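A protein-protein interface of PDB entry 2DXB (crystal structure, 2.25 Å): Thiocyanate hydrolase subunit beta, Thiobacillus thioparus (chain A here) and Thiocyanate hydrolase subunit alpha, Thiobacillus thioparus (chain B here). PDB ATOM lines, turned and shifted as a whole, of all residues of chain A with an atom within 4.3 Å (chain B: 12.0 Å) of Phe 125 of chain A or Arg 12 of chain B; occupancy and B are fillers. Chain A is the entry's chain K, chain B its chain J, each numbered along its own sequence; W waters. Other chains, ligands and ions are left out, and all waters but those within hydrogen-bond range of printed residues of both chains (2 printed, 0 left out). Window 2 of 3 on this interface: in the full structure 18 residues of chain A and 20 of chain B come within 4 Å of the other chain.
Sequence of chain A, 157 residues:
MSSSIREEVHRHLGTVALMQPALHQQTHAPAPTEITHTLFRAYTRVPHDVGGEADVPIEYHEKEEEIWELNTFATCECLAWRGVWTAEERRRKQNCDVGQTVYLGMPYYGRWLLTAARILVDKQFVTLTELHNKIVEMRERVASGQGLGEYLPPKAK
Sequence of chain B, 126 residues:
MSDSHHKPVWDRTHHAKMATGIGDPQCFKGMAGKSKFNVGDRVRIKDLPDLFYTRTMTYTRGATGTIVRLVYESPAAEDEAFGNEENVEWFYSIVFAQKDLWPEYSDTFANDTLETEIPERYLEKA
Of the 16 printed residues of chain B, 4 touch a printed residue of chain A.
Along chain B the printed residues that touch a printed residue of chain A span positions 7 to 12.
Of the 8 printed residues of chain A, 5 touch a printed residue of chain B.
Among the printed residues, 6 pairs touch across the chains.
Among the printed residues, no Asp or Glu carboxylate lies within 4 Å of a Lys or Arg side-chain nitrogen of the other chain.
The backbone carbonyl oxygen (O) of Val 84 of chain A lies within hydrogen-bond range of the side-chain amino group (NZ) of Lys 123 of chain A, 2.8 Å away.
The backbone NH (N) of Phe 125 of chain A is in hydrogen-bond range of the backbone carbonyl oxygen (O) of Leu 120 of chain A (2.8 Å).
Water W1 lies within hydrogen-bond range of the guanidinium group of Arg 12 of chain B and the backbone carbonyl oxygen of Arg 82 of chain A.
Water W2 lies within hydrogen-bond range of the backbone carbonyl oxygen (O) of Pro 8 of chain B (2.6 Å) and the side-chain amide oxygen (OE1) of Gln 124 of chain A (3.4 Å).
Among the printed residues, merely in contact across the chains: Gly 83 of chain A with Arg 12 of chain B, Gln 124 of chain A with Lys 7 of chain B, Gln 124 of chain A with Pro 8 of chain B and Phe 125 of chain A with Arg 12 of chain B.
Printed residues of chain B within 4 Å of Arg 82 of chain A: Arg 12 (3.4 Å).
Gly 83 of chain A touches one residue of chain B.
No residue of chain B comes within 4 Å of Val 84 of chain A.
No residue of chain B comes within 4 Å of Leu 120 of chain A.
Printed residues of chain B within 4 Å of Lys 123 of chain A: Trp 10.
Of chain B, only Lys 7 and Pro 8 come within 4 Å of Gln 124 of chain A.
Phe 125 of chain A touches just one residue of chain B: Arg 12.
Val 126 of chain A touches none of the printed residues of chain B.
Of the printed residues of chain A, Lys 7 of chain B touches Gln 124.
Printed residues of chain A within 4 Å of Pro 8 of chain B: Gln 124 (3.5 Å).
Of the printed residues of chain A, Trp 10 of chain B touches Lys 123 (3.4 Å).
Arg 12 of chain B touches just these residues of chain A: Arg 82 (3.4 Å), Gly 83 (3.3 Å) and Phe 125 (3.6 Å).
Ala 16 of chain B touches none of the printed residues of chain A.
The nearest residue of chain B that does not touch Phe 125 of chain A is Trp 10 of chain B (4.3 Å).
The nearest printed residue of chain A that does not touch Pro 8 of chain B is Lys 123 of chain A (5.6 Å).
NE1 of Trp 10 of chain B lies within hydrogen-bond range of O of Lys 123 of chain A, 3.4 Å away.
The backbone carbonyl oxygen (O) of Arg 82 of chain A sits close to the backbone carbonyl oxygen (O) of Arg 12 of chain B.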
ATOM      1  N   ARG A  82      10.783  14.112  13.499  1.00  0.00           N
ATOM      2  CA  ARG A  82      10.956  13.757  12.099  1.00  0.00           C
ATOM      3  C   ARG A  82      12.200  14.293  11.393  1.00  0.00           C
ATOM      4  O   ARG A  82      12.265  14.302  10.168  1.00  0.00           O
ATOM      5  CB  ARG A  82       9.689  14.124  11.312  1.00  0.00           C
ATOM      6  CG  ARG A  82       8.429  13.416  11.823  1.00  0.00           C
ATOM      7  CD  ARG A  82       8.695  11.929  12.112  1.00  0.00           C
ATOM      8  NE  ARG A  82       7.473  11.165  12.366  1.00  0.00           N
ATOM      9  CZ  ARG A  82       7.444   9.845  12.548  1.00  0.00           C
ATOM     10  NH1 ARG A  82       8.570   9.144  12.511  1.00  0.00           N
ATOM     11  NH2 ARG A  82       6.292   9.216  12.750  1.00  0.00           N
ATOM     12  N   GLY A  83      13.179  14.750  12.169  1.00  0.00           N
ATOM     13  CA  GLY A  83      14.433  15.211  11.596  1.00  0.00           C
ATOM     14  C   GLY A  83      14.563  16.552  10.904  1.00  0.00           C
ATOM     15  O   GLY A  83      15.532  16.761  10.176  1.00  0.00           O
ATOM     16  N   VAL A  84      13.614  17.459  11.102  1.00  0.00           N
ATOM     17  CA  VAL A  84      13.721  18.773  10.479  1.00  0.00           C
ATOM     18  C   VAL A  84      14.812  19.545  11.228  1.00  0.00           C
ATOM     19  O   VAL A  84      15.501  20.387  10.650  1.00  0.00           O
ATOM     20  CB  VAL A  84      12.377  19.541  10.536  1.00  0.00           C
ATOM     21  CG1 VAL A  84      12.581  21.001  10.140  1.00  0.00           C
ATOM     22  CG2 VAL A  84      11.382  18.892   9.586  1.00  0.00           C
ATOM     23  N   LEU A 120      11.172  26.222   8.947  1.00  0.00           N
ATOM     24  CA  LEU A 120      10.558  25.782   7.696  1.00  0.00           C
ATOM     25  C   LEU A 120      11.107  26.598   6.525  1.00  0.00           C
ATOM     26  O   LEU A 120      11.353  26.061   5.444  1.00  0.00           O
ATOM     27  CB  LEU A 120       9.035  25.949   7.734  1.00  0.00           C
ATOM     28  CG  LEU A 120       8.204  25.241   8.808  1.00  0.00           C
ATOM     29  CD1 LEU A 120       6.725  25.408   8.479  1.00  0.00           C
ATOM     30  CD2 LEU A 120       8.557  23.774   8.869  1.00  0.00           C
ATOM     31  N   LYS A 123      15.367  26.328   6.071  1.00  0.00           N
ATOM     32  CA  LYS A 123      15.805  25.085   5.447  1.00  0.00           C
ATOM     33  C   LYS A 123      15.062  24.827   4.139  1.00  0.00           C
ATOM     34  O   LYS A 123      15.116  23.736   3.571  1.00  0.00           O
ATOM     35  CB  LYS A 123      15.658  23.901   6.416  1.00  0.00           C
ATOM     36  CG  LYS A 123      16.867  23.776   7.353  1.00  0.00           C
ATOM     37  CD  LYS A 123      16.782  22.590   8.300  1.00  0.00           C
ATOM     38  CE  LYS A 123      18.079  22.454   9.095  1.00  0.00           C
ATOM     39  NZ  LYS A 123      18.011  21.401  10.157  1.00  0.00           N
ATOM     40  N   GLN A 124      14.368  25.858   3.671  1.00  0.00           N
ATOM     41  CA  GLN A 124      13.647  25.820   2.409  1.00  0.00           C
ATOM     42  C   GLN A 124      12.594  24.735   2.204  1.00  0.00           C
ATOM     43  O   GLN A 124      12.413  24.251   1.089  1.00  0.00           O
ATOM     44  CB  GLN A 124      14.660  25.781   1.259  1.00  0.00           C
ATOM     45  CG  GLN A 124      15.529  27.033   1.188  1.00  0.00           C
ATOM     46  CD  GLN A 124      16.618  26.940   0.134  1.00  0.00           C
ATOM     47  OE1 GLN A 124      17.490  26.078   0.204  1.00  0.00           O
ATOM     48  NE2 GLN A 124      16.568  27.830  -0.849  1.00  0.00           N
ATOM     49  N   PHE A 125      11.899  24.352   3.269  1.00  0.00           N
ATOM     50  CA  PHE A 125      10.840  23.361   3.139  1.00  0.00           C
ATOM     51  C   PHE A 125       9.613  24.113   2.620  1.00  0.00           C
ATOM     52  O   PHE A 125       8.707  23.533   2.023  1.00  0.00           O
ATOM     53  CB  PHE A 125      10.565  22.692   4.486  1.00  0.00           C
ATOM     54  CG  PHE A 125      11.669  21.771   4.930  1.00  0.00           C
ATOM     55  CD1 PHE A 125      11.997  20.648   4.175  1.00  0.00           C
ATOM     56  CD2 PHE A 125      12.393  22.033   6.086  1.00  0.00           C
ATOM     57  CE1 PHE A 125      13.032  19.800   4.563  1.00  0.00           C
ATOM     58  CE2 PHE A 125      13.431  21.190   6.484  1.00  0.00           C
ATOM     59  CZ  PHE A 125      13.750  20.073   5.720  1.00  0.00           C
ATOM     60  N   VAL A 126       9.599  25.420   2.860  1.00  0.00           N
ATOM     61  CA  VAL A 126       8.533  26.284   2.370  1.00  0.00           C
ATOM     62  C   VAL A 126       9.198  27.616   2.061  1.00  0.00           C
ATOM     63  O   VAL A 126      10.175  28.000   2.715  1.00  0.00           O
ATOM     64  CB  VAL A 126       7.405  26.528   3.416  1.00  0.00           C
ATOM     65  CG1 VAL A 126       6.982  25.216   4.048  1.00  0.00           C
ATOM     66  CG2 VAL A 126       7.860  27.522   4.468  1.00  0.00           C
ATOM     67  N   LYS B   7      18.714  22.773  -5.124  1.00  0.00           N
ATOM     68  CA  LYS B   7      18.629  23.171  -3.689  1.00  0.00           C
ATOM     69  C   LYS B   7      19.207  22.103  -2.769  1.00  0.00           C
ATOM     70  O   LYS B   7      19.180  20.913  -3.083  1.00  0.00           O
ATOM     71  CB  LYS B   7      17.174  23.441  -3.295  1.00  0.00           C
ATOM     72  CG  LYS B   7      16.581  24.693  -3.923  1.00  0.00           C
ATOM     73  CD  LYS B   7      15.184  24.978  -3.383  1.00  0.00           C
ATOM     74  CE  LYS B   7      14.638  26.285  -3.945  1.00  0.00           C
ATOM     75  NZ  LYS B   7      13.249  26.573  -3.479  1.00  0.00           N
ATOM     76  N   PRO B   8      19.743  22.521  -1.613  1.00  0.00           N
ATOM     77  CA  PRO B   8      20.325  21.584  -0.650  1.00  0.00           C
ATOM     78  C   PRO B   8      19.310  20.538  -0.205  1.00  0.00           C
ATOM     79  O   PRO B   8      18.112  20.815  -0.122  1.00  0.00           O
ATOM     80  CB  PRO B   8      20.749  22.493   0.501  1.00  0.00           C
ATOM     81  CG  PRO B   8      21.069  23.776  -0.188  1.00  0.00           C
ATOM     82  CD  PRO B   8      19.929  23.912  -1.165  1.00  0.00           C
ATOM     83  N   VAL B   9      19.796  19.336   0.072  1.00  0.00           N
ATOM     84  CA  VAL B   9      18.937  18.254   0.527  1.00  0.00           C
ATOM     85  C   VAL B   9      19.314  17.965   1.967  1.00  0.00           C
ATOM     86  O   VAL B   9      20.476  17.688   2.266  1.00  0.00           O
ATOM     87  CB  VAL B   9      19.147  16.975  -0.303  1.00  0.00           C
ATOM     88  CG1 VAL B   9      18.215  15.880   0.189  1.00  0.00           C
ATOM     89  CG2 VAL B   9      18.898  17.269  -1.770  1.00  0.00           C
ATOM     90  N   TRP B  10      18.338  18.043   2.863  1.00  0.00           N
ATOM     91  CA  TRP B  10      18.601  17.790   4.268  1.00  0.00           C
ATOM     92  C   TRP B  10      18.269  16.355   4.637  1.00  0.00           C
ATOM     93  O   TRP B  10      17.177  15.865   4.349  1.00  0.00           O
ATOM     94  CB  TRP B  10      17.800  18.753   5.145  1.00  0.00           C
ATOM     95  CG  TRP B  10      18.092  20.189   4.853  1.00  0.00           C
ATOM     96  CD1 TRP B  10      17.515  20.968   3.890  1.00  0.00           C
ATOM     97  CD2 TRP B  10      19.085  21.003   5.485  1.00  0.00           C
ATOM     98  NE1 TRP B  10      18.089  22.218   3.880  1.00  0.00           N
ATOM     99  CE2 TRP B  10      19.056  22.266   4.849  1.00  0.00           C
ATOM    100  CE3 TRP B  10      19.997  20.789   6.526  1.00  0.00           C
ATOM    101  CZ2 TRP B  10      19.906  23.311   5.222  1.00  0.00           C
ATOM    102  CZ3 TRP B  10      20.843  21.830   6.897  1.00  0.00           C
ATOM    103  CH2 TRP B  10      20.790  23.075   6.245  1.00  0.00           C
ATOM    104  N   ASP B  11      19.231  15.683   5.260  1.00  0.00           N
ATOM    105  CA  ASP B  11      19.054  14.305   5.693  1.00  0.00           C
ATOM    106  C   ASP B  11      18.159  14.339   6.930  1.00  0.00           C
ATOM    107  O   ASP B  11      18.613  14.685   8.021  1.00  0.00           O
ATOM    108  CB  ASP B  11      20.408  13.694   6.054  1.00  0.00           C
ATOM    109  CG  ASP B  11      20.301  12.241   6.466  1.00  0.00           C
ATOM    110  OD1 ASP B  11      19.357  11.905   7.211  1.00  0.00           O
ATOM    111  OD2 ASP B  11      21.163  11.437   6.054  1.00  0.00           O
ATOM    112  N   ARG B  12      16.893  13.977   6.767  1.00  0.00           N
ATOM    113  CA  ARG B  12      15.970  14.005   7.891  1.00  0.00           C
ATOM    114  C   ARG B  12      15.834  12.681   8.633  1.00  0.00           C
ATOM    115  O   ARG B  12      15.099  12.592   9.617  1.00  0.00           O
ATOM    116  CB  ARG B  12      14.592  14.479   7.421  1.00  0.00           C
ATOM    117  CG  ARG B  12      14.641  15.792   6.655  1.00  0.00           C
ATOM    118  CD  ARG B  12      13.404  16.637   6.895  1.00  0.00           C
ATOM    119  NE  ARG B  12      12.166  15.971   6.500  1.00  0.00           N
ATOM    120  CZ  ARG B  12      11.804  15.722   5.246  1.00  0.00           C
ATOM    121  NH1 ARG B  12      12.588  16.076   4.239  1.00  0.00           N
ATOM    122  NH2 ARG B  12      10.642  15.130   5.000  1.00  0.00           N
ATOM    123  N   THR B  13      16.554  11.658   8.180  1.00  0.00           N
ATOM    124  CA  THR B  13      16.471  10.344   8.812  1.00  0.00           C
ATOM    125  C   THR B  13      17.690   9.969   9.652  1.00  0.00           C
ATOM    126  O   THR B  13      17.621   9.049  10.462  1.00  0.00           O
ATOM    127  CB  THR B  13      16.272   9.238   7.758  1.00  0.00           C
ATOM    128  OG1 THR B  13      17.433   9.163   6.918  1.00  0.00           O
ATOM    129  CG2 THR B  13      15.049   9.531   6.905  1.00  0.00           C
ATOM    130  N   HIS B  14      18.798  10.677   9.461  1.00  0.00           N
ATOM    131  CA  HIS B  14      20.027  10.381  10.186  1.00  0.00           C
ATOM    132  C   HIS B  14      19.882  10.223  11.701  1.00  0.00           C
ATOM    133  O   HIS B  14      20.270   9.195  12.260  1.00  0.00           O
ATOM    134  CB  HIS B  14      21.082  11.450   9.902  1.00  0.00           C
ATOM    135  CG  HIS B  14      22.348  11.260  10.679  1.00  0.00           C
ATOM    136  ND1 HIS B  14      23.276  10.291  10.365  1.00  0.00           N
ATOM    137  CD2 HIS B  14      22.811  11.878  11.793  1.00  0.00           C
ATOM    138  CE1 HIS B  14      24.255  10.317  11.252  1.00  0.00           C
ATOM    139  NE2 HIS B  14      23.997  11.270  12.130  1.00  0.00           N
ATOM    140  N   HIS B  15      19.335  11.231  12.370  1.00  0.00           N
ATOM    141  CA  HIS B  15      19.201  11.158  13.821  1.00  0.00           C
ATOM    142  C   HIS B  15      18.381   9.962  14.295  1.00  0.00           C
ATOM    143  O   HIS B  15      18.813   9.222  15.180  1.00  0.00           O
ATOM    144  CB  HIS B  15      18.585  12.443  14.380  1.00  0.00           C
ATOM    145  CG  HIS B  15      18.621  12.520  15.874  1.00  0.00           C
ATOM    146  ND1 HIS B  15      19.795  12.646  16.585  1.00  0.00           N
ATOM    147  CD2 HIS B  15      17.629  12.453  16.794  1.00  0.00           C
ATOM    148  CE1 HIS B  15      19.527  12.654  17.878  1.00  0.00           C
ATOM    149  NE2 HIS B  15      18.221  12.538  18.032  1.00  0.00           N
ATOM    150  N   ALA B  16      17.201   9.777  13.710  1.00  0.00           N
ATOM    151  CA  ALA B  16      16.331   8.671  14.094  1.00  0.00           C
ATOM    152  C   ALA B  16      17.014   7.321  13.869  1.00  0.00           C
ATOM    153  O   ALA B  16      16.930   6.425  14.709  1.00  0.00           O
ATOM    154  CB  ALA B  16      15.015   8.738  13.311  1.00  0.00           C
ATOM    155  N   LYS B  17      17.691   7.179  12.735  1.00  0.00           N
ATOM    156  CA  LYS B  17      18.375   5.931  12.428  1.00  0.00           C
ATOM    157  C   LYS B  17      19.522   5.670  13.391  1.00  0.00           C
ATOM    158  O   LYS B  17      19.884   4.524  13.645  1.00  0.00           O
ATOM    159  CB  LYS B  17      18.913   5.954  10.996  1.00  0.00           C
ATOM    160  CG  LYS B  17      17.833   5.925   9.927  1.00  0.00           C
ATOM    161  CD  LYS B  17      18.442   5.987   8.538  1.00  0.00           C
ATOM    162  CE  LYS B  17      17.361   5.982   7.466  1.00  0.00           C
ATOM    163  NZ  LYS B  17      17.933   6.120   6.097  1.00  0.00           N
ATOM    164  N   MET B  18      20.090   6.736  13.935  1.00  0.00           N
ATOM    165  CA  MET B  18      21.209   6.605  14.852  1.00  0.00           C
ATOM    166  C   MET B  18      20.820   6.403  16.314  1.00  0.00           C
ATOM    167  O   MET B  18      21.517   5.707  17.047  1.00  0.00           O
ATOM    168  CB  MET B  18      22.112   7.839  14.731  1.00  0.00           C
ATOM    169  CG  MET B  18      23.141   7.976  15.835  1.00  0.00           C
ATOM    170  SD  MET B  18      24.259   9.353  15.547  1.00  0.00           S
ATOM    171  CE  MET B  18      23.148  10.749  15.822  1.00  0.00           C
ATOM    172  N   ALA B  19      19.705   6.991  16.733  1.00  0.00           N
ATOM    173  CA  ALA B  19      19.296   6.903  18.132  1.00  0.00           C
ATOM    174  C   ALA B  19      18.124   5.995  18.496  1.00  0.00           C
ATOM    175  O   ALA B  19      17.932   5.694  19.677  1.00  0.00           O
ATOM    176  CB  ALA B  19      19.023   8.317  18.663  1.00  0.00           C
ATOM    177  N   THR B  20      17.345   5.556  17.515  1.00  0.00           N
ATOM    178  CA  THR B  20      16.193   4.714  17.819  1.00  0.00           C
ATOM    179  C   THR B  20      16.551   3.493  18.656  1.00  0.00           C
ATOM    180  O   THR B  20      17.485   2.760  18.342  1.00  0.00           O
ATOM    181  CB  THR B  20      15.472   4.263  16.535  1.00  0.00           C
ATOM    182  OG1 THR B  20      14.947   5.414  15.866  1.00  0.00           O
ATOM    183  CG2 THR B  20      14.316   3.332  16.865  1.00  0.00           C
ATOM    184  N   GLY B  83      24.120  21.808  13.219  1.00  0.00           N
ATOM    185  CA  GLY B  83      24.108  20.598  12.416  1.00  0.00           C
ATOM    186  C   GLY B  83      25.432  19.887  12.223  1.00  0.00           C
ATOM    187  O   GLY B  83      25.552  19.036  11.346  1.00  0.00           O
ATOM    188  N   GLU B  85      27.753  17.324  13.796  1.00  0.00           N
ATOM    189  CA  GLU B  85      27.879  16.290  14.820  1.00  0.00           C
ATOM    190  C   GLU B  85      29.034  15.310  14.620  1.00  0.00           C
ATOM    191  O   GLU B  85      29.083  14.267  15.273  1.00  0.00           O
ATOM    192  CB  GLU B  85      26.566  15.503  14.912  1.00  0.00           C
ATOM    193  CG  GLU B  85      25.395  16.298  15.485  1.00  0.00           C
ATOM    194  CD  GLU B  85      24.070  15.553  15.392  1.00  0.00           C
ATOM    195  OE1 GLU B  85      24.058  14.316  15.578  1.00  0.00           O
ATOM    196  OE2 GLU B  85      23.033  16.205  15.142  1.00  0.00           O
HETATM  197  O   HOH W   1      10.368  14.952   8.006  1.00  0.00           O
HETATM  198  O   HOH W   2      16.455  22.835  -0.259  1.00  0.00           O
